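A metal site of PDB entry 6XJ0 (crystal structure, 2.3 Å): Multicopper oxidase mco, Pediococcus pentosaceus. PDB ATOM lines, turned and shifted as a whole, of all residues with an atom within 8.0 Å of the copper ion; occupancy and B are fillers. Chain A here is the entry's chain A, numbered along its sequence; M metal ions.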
ATOM      1  N   PRO A 209      31.247  17.798 -31.623  1.00  0.00           N
ATOM      2  CA  PRO A 209      30.648  19.036 -32.139  1.00  0.00           C
ATOM      3  C   PRO A 209      29.606  19.696 -31.236  1.00  0.00           C
ATOM      4  O   PRO A 209      29.290  20.880 -31.448  1.00  0.00           O
ATOM      5  CB  PRO A 209      29.993  18.580 -33.458  1.00  0.00           C
ATOM      6  CG  PRO A 209      29.744  17.131 -33.307  1.00  0.00           C
ATOM      7  CD  PRO A 209      30.841  16.619 -32.416  1.00  0.00           C
ATOM      8  N   ASP A 210      29.067  18.949 -30.271  1.00  0.00           N
ATOM      9  CA  ASP A 210      28.113  19.473 -29.301  1.00  0.00           C
ATOM     10  C   ASP A 210      28.738  20.109 -28.046  1.00  0.00           C
ATOM     11  O   ASP A 210      28.011  20.599 -27.167  1.00  0.00           O
ATOM     12  CB  ASP A 210      27.152  18.389 -28.819  1.00  0.00           C
ATOM     13  CG  ASP A 210      25.843  18.980 -28.283  1.00  0.00           C
ATOM     14  OD1 ASP A 210      25.367  19.950 -28.923  1.00  0.00           O
ATOM     15  OD2 ASP A 210      25.302  18.512 -27.250  1.00  0.00           O
ATOM     16  N   ARG A 244      32.266  23.807 -22.754  1.00  0.00           N
ATOM     17  CA  ARG A 244      30.830  23.576 -22.687  1.00  0.00           C
ATOM     18  C   ARG A 244      30.180  23.453 -21.325  1.00  0.00           C
ATOM     19  O   ARG A 244      29.001  23.787 -21.142  1.00  0.00           O
ATOM     20  CB  ARG A 244      30.455  22.348 -23.507  1.00  0.00           C
ATOM     21  CG  ARG A 244      28.953  22.317 -23.908  1.00  0.00           C
ATOM     22  CD  ARG A 244      28.272  21.257 -23.114  1.00  0.00           C
ATOM     23  NE  ARG A 244      26.833  21.105 -23.189  1.00  0.00           N
ATOM     24  CZ  ARG A 244      25.926  21.896 -22.612  1.00  0.00           C
ATOM     25  NH1 ARG A 244      24.642  21.546 -22.664  1.00  0.00           N
ATOM     26  NH2 ARG A 244      26.251  23.028 -21.992  1.00  0.00           N
ATOM     27  N   MET A 346      18.403  30.887 -32.479  1.00  0.00           N
ATOM     28  CA  MET A 346      19.365  29.820 -32.366  1.00  0.00           C
ATOM     29  C   MET A 346      18.677  28.479 -32.559  1.00  0.00           C
ATOM     30  O   MET A 346      17.684  28.183 -31.896  1.00  0.00           O
ATOM     31  CB  MET A 346      19.997  29.880 -30.987  1.00  0.00           C
ATOM     32  CG  MET A 346      20.964  31.034 -30.812  1.00  0.00           C
ATOM     33  SD  MET A 346      21.798  30.960 -29.192  1.00  0.00           S
ATOM     34  CE  MET A 346      20.360  31.319 -28.165  1.00  0.00           C
ATOM     35  N   GLN A 347      19.207  27.669 -33.474  1.00  0.00           N
ATOM     36  CA  GLN A 347      18.605  26.380 -33.823  1.00  0.00           C
ATOM     37  C   GLN A 347      19.664  25.318 -33.798  1.00  0.00           C
ATOM     38  O   GLN A 347      20.851  25.616 -34.053  1.00  0.00           O
ATOM     39  CB  GLN A 347      18.024  26.367 -35.233  1.00  0.00           C
ATOM     40  CG  GLN A 347      17.855  27.726 -35.854  1.00  0.00           C
ATOM     41  CD  GLN A 347      17.231  27.630 -37.223  1.00  0.00           C
ATOM     42  OE1 GLN A 347      17.776  26.979 -38.118  1.00  0.00           O
ATOM     43  NE2 GLN A 347      16.098  28.272 -37.387  1.00  0.00           N
ATOM     44  N   GLY A 348      19.235  24.092 -33.529  1.00  0.00           N
ATOM     45  CA  GLY A 348      20.082  22.916 -33.715  1.00  0.00           C
ATOM     46  C   GLY A 348      20.891  22.544 -32.493  1.00  0.00           C
ATOM     47  O   GLY A 348      20.915  23.261 -31.476  1.00  0.00           O
ATOM     48  N   MET A 349      21.512  21.370 -32.613  1.00  0.00           N
ATOM     49  CA  MET A 349      22.470  20.801 -31.638  1.00  0.00           C
ATOM     50  C   MET A 349      23.468  20.006 -32.445  1.00  0.00           C
ATOM     51  O   MET A 349      23.300  19.850 -33.649  1.00  0.00           O
ATOM     52  CB  MET A 349      21.778  19.871 -30.641  1.00  0.00           C
ATOM     53  CG  MET A 349      20.604  20.521 -29.910  1.00  0.00           C
ATOM     54  SD  MET A 349      19.910  19.574 -28.525  1.00  0.00           S
ATOM     55  CE  MET A 349      19.553  18.059 -29.414  1.00  0.00           C
ATOM     56  N   ASP A 350      24.531  19.530 -31.825  1.00  0.00           N
ATOM     57  CA  ASP A 350      25.577  18.816 -32.566  1.00  0.00           C
ATOM     58  C   ASP A 350      26.040  19.583 -33.832  1.00  0.00           C
ATOM     59  O   ASP A 350      26.322  20.783 -33.742  1.00  0.00           O
ATOM     60  CB  ASP A 350      25.139  17.364 -32.881  1.00  0.00           C
ATOM     61  CG  ASP A 350      24.789  16.550 -31.615  1.00  0.00           C
ATOM     62  OD1 ASP A 350      24.591  17.143 -30.536  1.00  0.00           O
ATOM     63  OD2 ASP A 350      24.696  15.309 -31.700  1.00  0.00           O
ATOM     64  N   VAL A 353      23.864  23.014 -35.607  1.00  0.00           N
ATOM     65  CA  VAL A 353      23.770  24.315 -35.060  1.00  0.00           C
ATOM     66  C   VAL A 353      23.899  25.407 -36.143  1.00  0.00           C
ATOM     67  O   VAL A 353      24.693  25.262 -37.103  1.00  0.00           O
ATOM     68  CB  VAL A 353      24.787  24.538 -33.963  1.00  0.00           C
ATOM     69  CG1 VAL A 353      24.566  23.560 -32.824  1.00  0.00           C
ATOM     70  CG2 VAL A 353      26.238  24.504 -34.508  1.00  0.00           C
ATOM     71  N   ALA A 354      23.120  26.475 -35.926  1.00  0.00           N
ATOM     72  CA  ALA A 354      22.953  27.554 -36.849  1.00  0.00           C
ATOM     73  C   ALA A 354      22.198  28.694 -36.148  1.00  0.00           C
ATOM     74  O   ALA A 354      21.670  28.527 -35.023  1.00  0.00           O
ATOM     75  CB  ALA A 354      22.143  27.082 -38.058  1.00  0.00           C
ATOM     76  N   ASN A 381      15.821  30.390 -28.396  1.00  0.00           N
ATOM     77  CA  ASN A 381      16.352  29.044 -28.548  1.00  0.00           C
ATOM     78  C   ASN A 381      15.168  28.114 -28.928  1.00  0.00           C
ATOM     79  O   ASN A 381      14.319  27.800 -28.107  1.00  0.00           O
ATOM     80  CB  ASN A 381      16.975  28.624 -27.225  1.00  0.00           C
ATOM     81  CG  ASN A 381      17.353  27.157 -27.144  1.00  0.00           C
ATOM     82  OD1 ASN A 381      17.247  26.372 -28.103  1.00  0.00           O
ATOM     83  ND2 ASN A 381      17.852  26.790 -25.948  1.00  0.00           N
ATOM     84  N   ASN A 383      15.226  24.951 -29.623  1.00  0.00           N
ATOM     85  CA  ASN A 383      15.313  23.565 -29.270  1.00  0.00           C
ATOM     86  C   ASN A 383      14.029  23.181 -28.591  1.00  0.00           C
ATOM     87  O   ASN A 383      13.405  23.974 -27.914  1.00  0.00           O
ATOM     88  CB  ASN A 383      16.464  23.255 -28.332  1.00  0.00           C
ATOM     89  CG  ASN A 383      17.839  23.394 -28.977  1.00  0.00           C
ATOM     90  OD1 ASN A 383      17.995  23.492 -30.193  1.00  0.00           O
ATOM     91  ND2 ASN A 383      18.838  23.415 -28.138  1.00  0.00           N
ATOM     92  N   MET A 388      18.926  21.831 -24.749  1.00  0.00           N
ATOM     93  CA  MET A 388      20.017  22.408 -23.963  1.00  0.00           C
ATOM     94  C   MET A 388      19.961  23.916 -23.852  1.00  0.00           C
ATOM     95  O   MET A 388      19.282  24.575 -24.614  1.00  0.00           O
ATOM     96  CB  MET A 388      21.344  21.979 -24.601  1.00  0.00           C
ATOM     97  CG  MET A 388      21.612  22.607 -25.970  1.00  0.00           C
ATOM     98  SD  MET A 388      22.803  21.869 -27.109  1.00  0.00           S
ATOM     99  CE  MET A 388      22.906  20.244 -26.443  1.00  0.00           C
ATOM    100  N   VAL A 389      20.722  24.456 -22.908  1.00  0.00           N
ATOM    101  CA  VAL A 389      20.833  25.913 -22.746  1.00  0.00           C
ATOM    102  C   VAL A 389      21.980  26.403 -23.628  1.00  0.00           C
ATOM    103  O   VAL A 389      23.099  25.876 -23.558  1.00  0.00           O
ATOM    104  CB  VAL A 389      21.088  26.287 -21.293  1.00  0.00           C
ATOM    105  CG1 VAL A 389      21.099  27.800 -21.089  1.00  0.00           C
ATOM    106  CG2 VAL A 389      20.045  25.652 -20.415  1.00  0.00           C
ATOM    107  N   HIS A 390      21.691  27.361 -24.485  1.00  0.00           N
ATOM    108  CA  HIS A 390      22.741  28.035 -25.267  1.00  0.00           C
ATOM    109  C   HIS A 390      23.024  29.445 -24.697  1.00  0.00           C
ATOM    110  O   HIS A 390      22.116  30.273 -24.544  1.00  0.00           O
ATOM    111  CB  HIS A 390      22.315  28.224 -26.711  1.00  0.00           C
ATOM    112  CG  HIS A 390      21.990  26.946 -27.432  1.00  0.00           C
ATOM    113  ND1 HIS A 390      22.916  26.252 -28.163  1.00  0.00           N
ATOM    114  CD2 HIS A 390      20.813  26.310 -27.626  1.00  0.00           C
ATOM    115  CE1 HIS A 390      22.362  25.199 -28.710  1.00  0.00           C
ATOM    116  NE2 HIS A 390      21.081  25.204 -28.401  1.00  0.00           N
ATOM    117  N   PRO A 391      24.283  29.708 -24.342  1.00  0.00           N
ATOM    118  CA  PRO A 391      24.636  30.999 -23.846  1.00  0.00           C
ATOM    119  C   PRO A 391      24.949  31.894 -25.016  1.00  0.00           C
ATOM    120  O   PRO A 391      25.928  31.677 -25.717  1.00  0.00           O
ATOM    121  CB  PRO A 391      25.869  30.703 -22.996  1.00  0.00           C
ATOM    122  CG  PRO A 391      26.479  29.510 -23.634  1.00  0.00           C
ATOM    123  CD  PRO A 391      25.342  28.710 -24.102  1.00  0.00           C
ATOM    124  N   PHE A 392      24.097  32.894 -25.213  1.00  0.00           N
ATOM    125  CA  PHE A 392      24.173  33.824 -26.355  1.00  0.00           C
ATOM    126  C   PHE A 392      25.027  35.046 -26.039  1.00  0.00           C
ATOM    127  O   PHE A 392      24.849  35.703 -24.989  1.00  0.00           O
ATOM    128  CB  PHE A 392      22.745  34.249 -26.726  1.00  0.00           C
ATOM    129  CG  PHE A 392      22.657  35.183 -27.902  1.00  0.00           C
ATOM    130  CD1 PHE A 392      22.799  34.710 -29.200  1.00  0.00           C
ATOM    131  CD2 PHE A 392      22.385  36.492 -27.708  1.00  0.00           C
ATOM    132  CE1 PHE A 392      22.730  35.562 -30.284  1.00  0.00           C
ATOM    133  CE2 PHE A 392      22.282  37.328 -28.773  1.00  0.00           C
ATOM    134  CZ  PHE A 392      22.452  36.870 -30.061  1.00  0.00           C
ATOM    135  N   VAL A 422      20.045  30.862 -22.631  1.00  0.00           N
ATOM    136  CA  VAL A 422      18.669  30.770 -23.146  1.00  0.00           C
ATOM    137  C   VAL A 422      18.199  29.316 -23.144  1.00  0.00           C
ATOM    138  O   VAL A 422      18.816  28.459 -23.771  1.00  0.00           O
ATOM    139  CB  VAL A 422      18.588  31.343 -24.554  1.00  0.00           C
ATOM    140  CG1 VAL A 422      17.157  31.689 -24.903  1.00  0.00           C
ATOM    141  CG2 VAL A 422      19.445  32.588 -24.676  1.00  0.00           C
ATOM    142  N   HIS A 443      26.831  35.188 -31.175  1.00  0.00           N
ATOM    143  CA  HIS A 443      26.896  33.741 -31.256  1.00  0.00           C
ATOM    144  C   HIS A 443      26.717  33.020 -29.966  1.00  0.00           C
ATOM    145  O   HIS A 443      26.876  33.615 -28.895  1.00  0.00           O
ATOM    146  CB  HIS A 443      28.291  33.342 -31.783  1.00  0.00           C
ATOM    147  CG  HIS A 443      29.426  33.787 -30.904  1.00  0.00           C
ATOM    148  ND1 HIS A 443      29.835  33.072 -29.796  1.00  0.00           N
ATOM    149  CD2 HIS A 443      30.248  34.859 -30.993  1.00  0.00           C
ATOM    150  CE1 HIS A 443      30.856  33.701 -29.236  1.00  0.00           C
ATOM    151  NE2 HIS A 443      31.163  34.737 -29.976  1.00  0.00           N
ATOM    152  N   CYS A 444      26.474  31.712 -30.079  1.00  0.00           N
ATOM    153  CA  CYS A 444      26.501  30.811 -28.901  1.00  0.00           C
ATOM    154  C   CYS A 444      27.933  30.679 -28.371  1.00  0.00           C
ATOM    155  O   CYS A 444      28.840  30.533 -29.170  1.00  0.00           O
ATOM    156  CB  CYS A 444      25.957  29.448 -29.256  1.00  0.00           C
ATOM    157  SG  CYS A 444      25.997  28.367 -27.827  1.00  0.00           S
ATOM    158  N   HIS A 445      28.142  30.804 -27.062  1.00  0.00           N
ATOM    159  CA  HIS A 445      29.483  30.731 -26.492  1.00  0.00           C
ATOM    160  C   HIS A 445      29.863  29.317 -25.916  1.00  0.00           C
ATOM    161  O   HIS A 445      30.841  29.166 -25.174  1.00  0.00           O
ATOM    162  CB  HIS A 445      29.681  31.833 -25.457  1.00  0.00           C
ATOM    163  CG  HIS A 445      31.090  32.325 -25.388  1.00  0.00           C
ATOM    164  ND1 HIS A 445      32.157  31.514 -25.087  1.00  0.00           N
ATOM    165  CD2 HIS A 445      31.624  33.548 -25.646  1.00  0.00           C
ATOM    166  CE1 HIS A 445      33.274  32.205 -25.121  1.00  0.00           C
ATOM    167  NE2 HIS A 445      32.976  33.457 -25.441  1.00  0.00           N
ATOM    168  N   ILE A 446      29.076  28.300 -26.243  1.00  0.00           N
ATOM    169  CA  ILE A 446      29.575  26.929 -26.247  1.00  0.00           C
ATOM    170  C   ILE A 446      30.521  26.889 -27.425  1.00  0.00           C
ATOM    171  O   ILE A 446      30.090  27.016 -28.570  1.00  0.00           O
ATOM    172  CB  ILE A 446      28.465  25.886 -26.411  1.00  0.00           C
ATOM    173  CG1 ILE A 446      27.617  25.892 -25.133  1.00  0.00           C
ATOM    174  CG2 ILE A 446      29.009  24.479 -26.687  1.00  0.00           C
ATOM    175  CD1 ILE A 446      26.475  24.918 -25.142  1.00  0.00           C
ATOM    176  N   ILE A 447      31.806  26.682 -27.152  1.00  0.00           N
ATOM    177  CA  ILE A 447      32.782  27.075 -28.143  1.00  0.00           C
ATOM    178  C   ILE A 447      32.777  26.161 -29.380  1.00  0.00           C
ATOM    179  O   ILE A 447      33.056  26.607 -30.512  1.00  0.00           O
ATOM    180  CB  ILE A 447      34.196  27.275 -27.549  1.00  0.00           C
ATOM    181  CG1 ILE A 447      34.152  28.027 -26.193  1.00  0.00           C
ATOM    182  CG2 ILE A 447      35.018  28.114 -28.494  1.00  0.00           C
ATOM    183  CD1 ILE A 447      35.528  28.226 -25.552  1.00  0.00           C
ATOM    184  N   GLU A 448      32.443  24.900 -29.188  1.00  0.00           N
ATOM    185  CA  GLU A 448      32.228  23.997 -30.361  1.00  0.00           C
ATOM    186  C   GLU A 448      31.048  24.419 -31.279  1.00  0.00           C
ATOM    187  O   GLU A 448      31.057  24.216 -32.503  1.00  0.00           O
ATOM    188  CB  GLU A 448      32.016  22.572 -29.881  1.00  0.00           C
ATOM    189  CG  GLU A 448      33.319  21.890 -29.452  1.00  0.00           C
ATOM    190  CD  GLU A 448      33.959  22.439 -28.161  1.00  0.00           C
ATOM    191  OE1 GLU A 448      33.219  22.630 -27.140  1.00  0.00           O
ATOM    192  OE2 GLU A 448      35.211  22.624 -28.113  1.00  0.00           O
ATOM    193  N   HIS A 449      30.011  25.021 -30.686  1.00  0.00           N
ATOM    194  CA  HIS A 449      28.880  25.544 -31.467  1.00  0.00           C
ATOM    195  C   HIS A 449      29.260  26.746 -32.308  1.00  0.00           C
ATOM    196  O   HIS A 449      28.913  26.826 -33.493  1.00  0.00           O
ATOM    197  CB  HIS A 449      27.739  25.927 -30.551  1.00  0.00           C
ATOM    198  CG  HIS A 449      27.044  24.764 -29.968  1.00  0.00           C
ATOM    199  ND1 HIS A 449      25.857  24.893 -29.295  1.00  0.00           N
ATOM    200  CD2 HIS A 449      27.349  23.448 -29.964  1.00  0.00           C
ATOM    201  CE1 HIS A 449      25.456  23.695 -28.895  1.00  0.00           C
ATOM    202  NE2 HIS A 449      26.359  22.806 -29.284  1.00  0.00           N
ATOM    203  N   GLU A 450      29.940  27.683 -31.670  1.00  0.00           N
ATOM    204  CA  GLU A 450      30.558  28.820 -32.329  1.00  0.00           C
ATOM    205  C   GLU A 450      31.443  28.418 -33.525  1.00  0.00           C
ATOM    206  O   GLU A 450      31.205  28.847 -34.646  1.00  0.00           O
ATOM    207  CB  GLU A 450      31.368  29.556 -31.244  1.00  0.00           C
ATOM    208  CG  GLU A 450      32.477  30.495 -31.657  1.00  0.00           C
ATOM    209  CD  GLU A 450      33.047  31.252 -30.456  1.00  0.00           C
ATOM    210  OE1 GLU A 450      32.563  31.076 -29.292  1.00  0.00           O
ATOM    211  OE2 GLU A 450      34.019  32.029 -30.662  1.00  0.00           O
ATOM    212  N   MET A 454      27.261  28.191 -35.184  1.00  0.00           N
ATOM    213  CA  MET A 454      26.258  28.964 -34.488  1.00  0.00           C
ATOM    214  C   MET A 454      26.752  30.363 -34.202  1.00  0.00           C
ATOM    215  O   MET A 454      26.946  30.789 -33.062  1.00  0.00           O
ATOM    216  CB  MET A 454      25.858  28.283 -33.201  1.00  0.00           C
ATOM    217  CG  MET A 454      24.461  28.687 -32.738  1.00  0.00           C
ATOM    218  SD  MET A 454      24.108  27.625 -31.321  1.00  0.00           S
ATOM    219  CE  MET A 454      22.540  26.904 -31.788  1.00  0.00           C
HETATM  220 CU    CU M   1      24.890  26.592 -28.566  1.00  0.00          CU
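The nearest printed residue that does not touch the copper ion is Ile 446 (4.1 Å).
The side-chain sulfur (SD) of Met 454 lies close to a ring nitrogen (ND1) of His 390 (3.6 Å). A ring nitrogen (NE2) of His 390 sits at hydrogen-bond distance from the side-chain amide nitrogen of Asn 383. O of His 390 sits at hydrogen-bond distance from N of Val 422 (2.9 Å). N of Met 454 is in hydrogen-bond range of O of His 449, at 2.7 Å. NE2 of His 449 lies within hydrogen-bond range of OD1 of Asp 210, 3.0 Å away. N of Cys 444 is in hydrogen-bond range of O of Met 454 (3.2 Å). SG of Cys 444 lies close to N of Ile 446.
The copper ion is bound by a ring nitrogen (ND1) of His 390, a ring nitrogen (ND1) of His 449 and the side-chain sulfur (SG) of Cys 444. The copper ion has three donor atoms within binding distance. Slightly farther from the copper ion lies the side-chain sulfur (SD) of Met 454 (3.0 Å).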
